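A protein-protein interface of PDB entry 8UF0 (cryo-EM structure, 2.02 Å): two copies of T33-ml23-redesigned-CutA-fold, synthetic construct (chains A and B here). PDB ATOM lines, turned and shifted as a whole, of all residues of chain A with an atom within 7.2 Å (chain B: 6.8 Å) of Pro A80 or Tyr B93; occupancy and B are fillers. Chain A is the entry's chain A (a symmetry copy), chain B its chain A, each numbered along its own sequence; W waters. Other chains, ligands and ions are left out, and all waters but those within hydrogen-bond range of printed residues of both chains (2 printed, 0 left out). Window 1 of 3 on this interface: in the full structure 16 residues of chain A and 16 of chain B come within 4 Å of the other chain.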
ATOM      1  N   ILE A   4     -18.354   6.424  20.427  1.00  0.00           N
ATOM      2  CA  ILE A   4     -17.903   7.746  20.863  1.00  0.00           C
ATOM      3  C   ILE A   4     -16.432   7.922  20.487  1.00  0.00           C
ATOM      4  O   ILE A   4     -15.615   7.042  20.764  1.00  0.00           O
ATOM      5  CB  ILE A   4     -18.108   7.931  22.381  1.00  0.00           C
ATOM      6  CG1 ILE A   4     -19.574   7.727  22.768  1.00  0.00           C
ATOM      7  CG2 ILE A   4     -17.618   9.294  22.849  1.00  0.00           C
ATOM      8  CD1 ILE A   4     -19.796   7.541  24.234  1.00  0.00           C
ATOM      9  N   GLU A   5     -16.091   9.067  19.883  1.00  0.00           N
ATOM     10  CA  GLU A   5     -14.733   9.358  19.417  1.00  0.00           C
ATOM     11  C   GLU A   5     -14.192  10.674  19.974  1.00  0.00           C
ATOM     12  O   GLU A   5     -14.929  11.654  20.078  1.00  0.00           O
ATOM     13  CB  GLU A   5     -14.681   9.433  17.893  1.00  0.00           C
ATOM     14  CG  GLU A   5     -15.232   8.234  17.187  1.00  0.00           C
ATOM     15  CD  GLU A   5     -14.292   7.708  16.133  1.00  0.00           C
ATOM     16  OE1 GLU A   5     -13.157   7.329  16.485  1.00  0.00           O
ATOM     17  OE2 GLU A   5     -14.682   7.679  14.949  1.00  0.00           O
ATOM     18  N   THR A   6     -12.892  10.699  20.284  1.00  0.00           N
ATOM     19  CA  THR A   6     -12.187  11.904  20.719  1.00  0.00           C
ATOM     20  C   THR A   6     -10.691  11.738  20.443  1.00  0.00           C
ATOM     21  O   THR A   6     -10.243  10.675  20.018  1.00  0.00           O
ATOM     22  CB  THR A   6     -12.479  12.217  22.204  1.00  0.00           C
ATOM     23  OG1 THR A   6     -12.041  13.541  22.525  1.00  0.00           O
ATOM     24  CG2 THR A   6     -11.816  11.231  23.136  1.00  0.00           C
ATOM     25  N   THR A   7      -9.918  12.808  20.672  1.00  0.00           N
ATOM     26  CA  THR A   7      -8.468  12.819  20.457  1.00  0.00           C
ATOM     27  C   THR A   7      -7.743  13.473  21.633  1.00  0.00           C
ATOM     28  O   THR A   7      -8.310  14.295  22.346  1.00  0.00           O
ATOM     29  CB  THR A   7      -8.063  13.556  19.151  1.00  0.00           C
ATOM     30  OG1 THR A   7      -8.557  14.896  19.157  1.00  0.00           O
ATOM     31  CG2 THR A   7      -8.578  12.847  17.913  1.00  0.00           C
ATOM     32  N   THR A   8      -6.477  13.110  21.823  1.00  0.00           N
ATOM     33  CA  THR A   8      -5.622  13.629  22.883  1.00  0.00           C
ATOM     34  C   THR A   8      -4.217  13.887  22.352  1.00  0.00           C
ATOM     35  O   THR A   8      -3.828  13.335  21.320  1.00  0.00           O
ATOM     36  CB  THR A   8      -5.522  12.684  24.097  1.00  0.00           C
ATOM     37  OG1 THR A   8      -4.874  11.464  23.725  1.00  0.00           O
ATOM     38  CG2 THR A   8      -6.882  12.387  24.704  1.00  0.00           C
ATOM     39  N   LYS A  38      -2.376  16.274  12.743  1.00  0.00           N
ATOM     40  CA  LYS A  38      -3.492  17.210  12.731  1.00  0.00           C
ATOM     41  C   LYS A  38      -3.057  18.545  12.129  1.00  0.00           C
ATOM     42  O   LYS A  38      -1.973  19.041  12.431  1.00  0.00           O
ATOM     43  CB  LYS A  38      -4.039  17.431  14.142  1.00  0.00           C
ATOM     44  CG  LYS A  38      -5.138  18.460  14.204  1.00  0.00           C
ATOM     45  CD  LYS A  38      -6.006  18.320  15.419  1.00  0.00           C
ATOM     46  CE  LYS A  38      -5.618  19.316  16.476  1.00  0.00           C
ATOM     47  NZ  LYS A  38      -6.576  19.297  17.604  1.00  0.00           N
ATOM     48  N   ILE A  70     -16.401  12.155  30.478  1.00  0.00           N
ATOM     49  CA  ILE A  70     -15.254  12.477  29.629  1.00  0.00           C
ATOM     50  C   ILE A  70     -14.948  13.972  29.680  1.00  0.00           C
ATOM     51  O   ILE A  70     -13.785  14.375  29.771  1.00  0.00           O
ATOM     52  CB  ILE A  70     -15.489  11.996  28.182  1.00  0.00           C
ATOM     53  CG1 ILE A  70     -15.436  10.471  28.096  1.00  0.00           C
ATOM     54  CG2 ILE A  70     -14.457  12.577  27.237  1.00  0.00           C
ATOM     55  CD1 ILE A  70     -16.039   9.926  26.841  1.00  0.00           C
ATOM     56  N   HIS A  74     -10.976  15.405  30.630  1.00  0.00           N
ATOM     57  CA  HIS A  74     -10.177  15.586  29.419  1.00  0.00           C
ATOM     58  C   HIS A  74      -9.115  16.672  29.611  1.00  0.00           C
ATOM     59  O   HIS A  74      -9.367  17.678  30.267  1.00  0.00           O
ATOM     60  CB  HIS A  74     -11.083  15.956  28.246  1.00  0.00           C
ATOM     61  CG  HIS A  74     -10.484  15.696  26.901  1.00  0.00           C
ATOM     62  ND1 HIS A  74      -9.465  16.461  26.379  1.00  0.00           N
ATOM     63  CD2 HIS A  74     -10.777  14.771  25.958  1.00  0.00           C
ATOM     64  CE1 HIS A  74      -9.144  16.006  25.185  1.00  0.00           C
ATOM     65  NE2 HIS A  74      -9.928  14.983  24.905  1.00  0.00           N
ATOM     66  N   ASP A  76      -7.835  18.807  27.265  1.00  0.00           N
ATOM     67  CA  ASP A  76      -7.876  20.032  26.465  1.00  0.00           C
ATOM     68  C   ASP A  76      -8.973  20.986  26.937  1.00  0.00           C
ATOM     69  O   ASP A  76      -9.996  20.552  27.468  1.00  0.00           O
ATOM     70  CB  ASP A  76      -8.105  19.705  24.990  1.00  0.00           C
ATOM     71  CG  ASP A  76      -6.966  18.915  24.374  1.00  0.00           C
ATOM     72  OD1 ASP A  76      -5.835  18.973  24.895  1.00  0.00           O
ATOM     73  OD2 ASP A  76      -7.201  18.233  23.360  1.00  0.00           O
ATOM     74  N   ILE A  78     -11.185  22.793  25.162  1.00  0.00           N
ATOM     75  CA  ILE A  78     -12.453  22.527  24.479  1.00  0.00           C
ATOM     76  C   ILE A  78     -12.368  21.178  23.772  1.00  0.00           C
ATOM     77  O   ILE A  78     -11.963  21.117  22.605  1.00  0.00           O
ATOM     78  CB  ILE A  78     -12.821  23.643  23.487  1.00  0.00           C
ATOM     79  CG1 ILE A  78     -12.765  25.016  24.154  1.00  0.00           C
ATOM     80  CG2 ILE A  78     -14.206  23.403  22.913  1.00  0.00           C
ATOM     81  CD1 ILE A  78     -13.280  26.135  23.299  1.00  0.00           C
ATOM     82  N   PRO A  79     -12.736  20.083  24.422  1.00  0.00           N
ATOM     83  CA  PRO A  79     -12.505  18.755  23.840  1.00  0.00           C
ATOM     84  C   PRO A  79     -13.518  18.419  22.763  1.00  0.00           C
ATOM     85  O   PRO A  79     -14.723  18.641  22.930  1.00  0.00           O
ATOM     86  CB  PRO A  79     -12.639  17.817  25.045  1.00  0.00           C
ATOM     87  CG  PRO A  79     -13.488  18.529  25.977  1.00  0.00           C
ATOM     88  CD  PRO A  79     -13.257  20.001  25.791  1.00  0.00           C
ATOM     89  N   PRO A  80     -13.066  17.870  21.636  1.00  0.00           N
ATOM     90  CA  PRO A  80     -13.989  17.380  20.602  1.00  0.00           C
ATOM     91  C   PRO A  80     -14.509  15.991  20.953  1.00  0.00           C
ATOM     92  O   PRO A  80     -13.733  15.054  21.122  1.00  0.00           O
ATOM     93  CB  PRO A  80     -13.121  17.354  19.341  1.00  0.00           C
ATOM     94  CG  PRO A  80     -11.727  17.304  19.821  1.00  0.00           C
ATOM     95  CD  PRO A  80     -11.656  17.728  21.244  1.00  0.00           C
ATOM     96  N   ILE A  81     -15.825  15.864  21.075  1.00  0.00           N
ATOM     97  CA  ILE A  81     -16.476  14.605  21.410  1.00  0.00           C
ATOM     98  C   ILE A  81     -17.650  14.408  20.460  1.00  0.00           C
ATOM     99  O   ILE A  81     -18.523  15.272  20.374  1.00  0.00           O
ATOM    100  CB  ILE A  81     -16.952  14.579  22.877  1.00  0.00           C
ATOM    101  CG1 ILE A  81     -15.793  14.878  23.832  1.00  0.00           C
ATOM    102  CG2 ILE A  81     -17.587  13.249  23.212  1.00  0.00           C
ATOM    103  CD1 ILE A  81     -16.221  15.320  25.196  1.00  0.00           C
ATOM    104  N   ILE A  82     -17.687  13.264  19.778  1.00  0.00           N
ATOM    105  CA  ILE A  82     -18.640  13.003  18.703  1.00  0.00           C
ATOM    106  C   ILE A  82     -19.261  11.619  18.881  1.00  0.00           C
ATOM    107  O   ILE A  82     -18.571  10.668  19.254  1.00  0.00           O
ATOM    108  CB  ILE A  82     -17.940  13.147  17.333  1.00  0.00           C
ATOM    109  CG1 ILE A  82     -17.796  14.620  16.977  1.00  0.00           C
ATOM    110  CG2 ILE A  82     -18.678  12.429  16.240  1.00  0.00           C
ATOM    111  CD1 ILE A  82     -16.512  14.944  16.309  1.00  0.00           C
ATOM    112  N   ALA B  28     -12.708  23.393   9.305  1.00  0.00           N
ATOM    113  CA  ALA B  28     -12.060  23.841  10.532  1.00  0.00           C
ATOM    114  C   ALA B  28     -10.767  23.097  10.866  1.00  0.00           C
ATOM    115  O   ALA B  28      -9.841  23.721  11.378  1.00  0.00           O
ATOM    116  CB  ALA B  28     -13.032  23.738  11.708  1.00  0.00           C
ATOM    117  N   GLU B  29     -10.669  21.790  10.608  1.00  0.00           N
ATOM    118  CA  GLU B  29      -9.433  21.041  10.848  1.00  0.00           C
ATOM    119  C   GLU B  29      -9.475  19.707  10.100  1.00  0.00           C
ATOM    120  O   GLU B  29     -10.524  19.282   9.619  1.00  0.00           O
ATOM    121  CB  GLU B  29      -9.182  20.816  12.349  1.00  0.00           C
ATOM    122  CG  GLU B  29     -10.295  20.124  13.099  1.00  0.00           C
ATOM    123  CD  GLU B  29     -10.001  19.970  14.591  1.00  0.00           C
ATOM    124  OE1 GLU B  29      -8.970  20.491  15.063  1.00  0.00           O
ATOM    125  OE2 GLU B  29     -10.807  19.336  15.301  1.00  0.00           O
ATOM    126  N   TYR B  57     -13.500  17.932   9.169  1.00  0.00           N
ATOM    127  CA  TYR B  57     -14.577  18.312  10.081  1.00  0.00           C
ATOM    128  C   TYR B  57     -15.113  19.692   9.719  1.00  0.00           C
ATOM    129  O   TYR B  57     -14.343  20.650   9.621  1.00  0.00           O
ATOM    130  CB  TYR B  57     -14.083  18.297  11.535  1.00  0.00           C
ATOM    131  CG  TYR B  57     -13.528  16.964  11.979  1.00  0.00           C
ATOM    132  CD1 TYR B  57     -12.217  16.603  11.694  1.00  0.00           C
ATOM    133  CD2 TYR B  57     -14.322  16.053  12.660  1.00  0.00           C
ATOM    134  CE1 TYR B  57     -11.714  15.387  12.077  1.00  0.00           C
ATOM    135  CE2 TYR B  57     -13.825  14.831  13.052  1.00  0.00           C
ATOM    136  CZ  TYR B  57     -12.521  14.505  12.761  1.00  0.00           C
ATOM    137  OH  TYR B  57     -12.021  13.293  13.148  1.00  0.00           O
ATOM    138  N   ALA B  89     -22.973  15.755  19.791  1.00  0.00           N
ATOM    139  CA  ALA B  89     -21.653  16.367  19.937  1.00  0.00           C
ATOM    140  C   ALA B  89     -21.662  17.336  21.114  1.00  0.00           C
ATOM    141  O   ALA B  89     -22.710  17.864  21.490  1.00  0.00           O
ATOM    142  CB  ALA B  89     -21.230  17.089  18.654  1.00  0.00           C
ATOM    143  N   ASN B  90     -20.479  17.570  21.681  1.00  0.00           N
ATOM    144  CA  ASN B  90     -20.279  18.553  22.746  1.00  0.00           C
ATOM    145  C   ASN B  90     -20.649  19.946  22.238  1.00  0.00           C
ATOM    146  O   ASN B  90     -20.059  20.411  21.258  1.00  0.00           O
ATOM    147  CB  ASN B  90     -18.819  18.511  23.213  1.00  0.00           C
ATOM    148  CG  ASN B  90     -18.483  19.567  24.268  1.00  0.00           C
ATOM    149  OD1 ASN B  90     -19.355  20.127  24.919  1.00  0.00           O
ATOM    150  ND2 ASN B  90     -17.200  19.828  24.440  1.00  0.00           N
ATOM    151  N   PRO B  91     -21.609  20.633  22.862  1.00  0.00           N
ATOM    152  CA  PRO B  91     -22.043  21.940  22.332  1.00  0.00           C
ATOM    153  C   PRO B  91     -20.947  22.995  22.273  1.00  0.00           C
ATOM    154  O   PRO B  91     -20.969  23.834  21.370  1.00  0.00           O
ATOM    155  CB  PRO B  91     -23.172  22.344  23.289  1.00  0.00           C
ATOM    156  CG  PRO B  91     -23.659  21.059  23.853  1.00  0.00           C
ATOM    157  CD  PRO B  91     -22.457  20.184  23.977  1.00  0.00           C
ATOM    158  N   ALA B  92     -19.991  22.977  23.198  1.00  0.00           N
ATOM    159  CA  ALA B  92     -18.895  23.938  23.143  1.00  0.00           C
ATOM    160  C   ALA B  92     -18.036  23.740  21.895  1.00  0.00           C
ATOM    161  O   ALA B  92     -17.539  24.710  21.319  1.00  0.00           O
ATOM    162  CB  ALA B  92     -18.044  23.840  24.406  1.00  0.00           C
ATOM    163  N   TYR B  93     -17.849  22.490  21.466  1.00  0.00           N
ATOM    164  CA  TYR B  93     -17.057  22.228  20.267  1.00  0.00           C
ATOM    165  C   TYR B  93     -17.768  22.707  19.004  1.00  0.00           C
ATOM    166  O   TYR B  93     -17.123  23.212  18.083  1.00  0.00           O
ATOM    167  CB  TYR B  93     -16.714  20.739  20.179  1.00  0.00           C
ATOM    168  CG  TYR B  93     -15.853  20.364  18.994  1.00  0.00           C
ATOM    169  CD1 TYR B  93     -14.512  20.697  18.956  1.00  0.00           C
ATOM    170  CD2 TYR B  93     -16.384  19.674  17.919  1.00  0.00           C
ATOM    171  CE1 TYR B  93     -13.732  20.367  17.888  1.00  0.00           C
ATOM    172  CE2 TYR B  93     -15.603  19.332  16.843  1.00  0.00           C
ATOM    173  CZ  TYR B  93     -14.277  19.680  16.838  1.00  0.00           C
ATOM    174  OH  TYR B  93     -13.495  19.348  15.768  1.00  0.00           O
ATOM    175  N   LYS B  94     -19.093  22.575  18.945  1.00  0.00           N
ATOM    176  CA  LYS B  94     -19.834  23.120  17.810  1.00  0.00           C
ATOM    177  C   LYS B  94     -19.701  24.634  17.732  1.00  0.00           C
ATOM    178  O   LYS B  94     -19.643  25.201  16.638  1.00  0.00           O
ATOM    179  CB  LYS B  94     -21.305  22.721  17.882  1.00  0.00           C
ATOM    180  CG  LYS B  94     -21.561  21.327  17.393  1.00  0.00           C
ATOM    181  CD  LYS B  94     -22.640  20.641  18.177  1.00  0.00           C
ATOM    182  CE  LYS B  94     -23.998  21.025  17.659  1.00  0.00           C
ATOM    183  NZ  LYS B  94     -24.086  20.809  16.193  1.00  0.00           N
ATOM    184  N   GLY B  95     -19.645  25.304  18.882  1.00  0.00           N
ATOM    185  CA  GLY B  95     -19.370  26.728  18.883  1.00  0.00           C
ATOM    186  C   GLY B  95     -18.013  27.075  18.300  1.00  0.00           C
ATOM    187  O   GLY B  95     -17.888  28.032  17.539  1.00  0.00           O
ATOM    188  N   TRP B  96     -16.978  26.309  18.653  1.00  0.00           N
ATOM    189  CA  TRP B  96     -15.647  26.571  18.109  1.00  0.00           C
ATOM    190  C   TRP B  96     -15.603  26.349  16.598  1.00  0.00           C
ATOM    191  O   TRP B  96     -14.979  27.126  15.872  1.00  0.00           O
ATOM    192  CB  TRP B  96     -14.600  25.705  18.816  1.00  0.00           C
ATOM    193  CG  TRP B  96     -13.207  25.908  18.296  1.00  0.00           C
ATOM    194  CD1 TRP B  96     -12.350  26.907  18.627  1.00  0.00           C
ATOM    195  CD2 TRP B  96     -12.525  25.101  17.332  1.00  0.00           C
ATOM    196  NE1 TRP B  96     -11.178  26.776  17.939  1.00  0.00           N
ATOM    197  CE2 TRP B  96     -11.258  25.673  17.135  1.00  0.00           C
ATOM    198  CE3 TRP B  96     -12.862  23.949  16.621  1.00  0.00           C
ATOM    199  CZ2 TRP B  96     -10.323  25.132  16.256  1.00  0.00           C
ATOM    200  CZ3 TRP B  96     -11.934  23.413  15.751  1.00  0.00           C
ATOM    201  CH2 TRP B  96     -10.680  24.004  15.575  1.00  0.00           C
ATOM    202  N   VAL B  97     -16.272  25.303  16.106  1.00  0.00           N
ATOM    203  CA  VAL B  97     -16.273  25.018  14.672  1.00  0.00           C
ATOM    204  C   VAL B  97     -16.932  26.153  13.894  1.00  0.00           C
ATOM    205  O   VAL B  97     -16.421  26.589  12.860  1.00  0.00           O
ATOM    206  CB  VAL B  97     -16.954  23.662  14.392  1.00  0.00           C
ATOM    207  CG1 VAL B  97     -17.341  23.536  12.923  1.00  0.00           C
ATOM    208  CG2 VAL B  97     -16.055  22.514  14.799  1.00  0.00           C
ATOM    209  N   ALA B  98     -18.065  26.662  14.386  1.00  0.00           N
ATOM    210  CA  ALA B  98     -18.728  27.781  13.720  1.00  0.00           C
ATOM    211  C   ALA B  98     -17.883  29.051  13.764  1.00  0.00           C
ATOM    212  O   ALA B  98     -17.862  29.818  12.801  1.00  0.00           O
ATOM    213  CB  ALA B  98     -20.102  28.026  14.339  1.00  0.00           C
HETATM  214  O   HOH W   1      -9.415  16.900  17.177  1.00  0.00           O
HETATM  215  O   HOH W   2      -9.554  20.246  18.121  1.00  0.00           O
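The backbone NH of Asn B90 sits at hydrogen-bond distance from the backbone carbonyl oxygen of Ile A81, 3.3 Å away.
OE1 of Glu B29 lies within salt-bridge range of NZ of Lys A38 (3.7 Å).
ND2 of Asn B90 lies within hydrogen-bond range of O of Pro A79 (3.1 Å).
O of Glu B29 sits at hydrogen-bond distance from N of Tyr B57 (3.3 Å).
The backbone NH (N) of Ala B92 sits close to the side-chain amide oxygen (OD1) of Asn B90.
O of Pro A80 is in hydrogen-bond range of OG1 of Thr A6 (2.7 Å).
OE2 of Glu B29 sits at hydrogen-bond distance from OH of Tyr B93, at 2.7 Å.
O of Ala B92 touches CG2 of Ile A78 (3.9 Å).
Pro A79 touches Tyr B93.
Tyr B93 touches Pro A80 (CE1 to CB, 3.4 Å).
Ile A81 touches Ala B89.
Pro A80 touches just one residue of chain B: Tyr B93 (3.4 Å).
Of the printed residues of chain A, Tyr B93 touches Pro A79 (3.99 Å) and Pro A80 (3.4 Å).
Of the printed residues of chain A, Glu B29 touches Lys A38.
Of the printed residues of chain B, Ile A78 touches Ala B92 (3.9 Å).
Of the printed residues of chain A, Ala B89 touches Ile A81 (3.3 Å).
Of the printed residues of chain B, Pro A79 touches Asn B90 (3.1 Å) and Tyr B93 (3.99 Å).
Printed residues of chain A within 4 Å of Ala B92: Ile A78.
The nearest residue of chain B that does not touch Pro A80 is Glu B29 (5.0 Å).
The nearest printed residue of chain A that does not touch Tyr B93 is Ile A78 (4.02 Å).
Of the 14 printed residues of chain A, 5 touch a printed residue of chain B.
Printed residues of chain A that touch a printed residue of chain B: Lys A38, Ile A78, Pro A79, Pro A80 and Ile A81.
Hydrophobic or aromatic side chains of chain A within 4 Å of the printed part of chain B: Ile A78 and Pro A80.
Along chain A the printed residues that touch a printed residue of chain B span positions 38 to 81.
Among the printed residues, Asp or Glu carboxylates within 4 Å of a Lys or Arg side-chain nitrogen of the other chain: Lys A38 with Glu B29 (3.7 Å).
No position is printed for both chains.
Of the 7 pairs that touch across the chains among the printed residues, none has its exchanged pair printed and touching as well.
Water W1 lies within hydrogen-bond range of the side-chain hydroxyl of Thr A7 (2.9 Å) and the side-chain carboxylate of Glu B29 (3.4 Å).
Water W2 lies within hydrogen-bond range of OE1 of Glu B29 and NZ of Lys A38.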
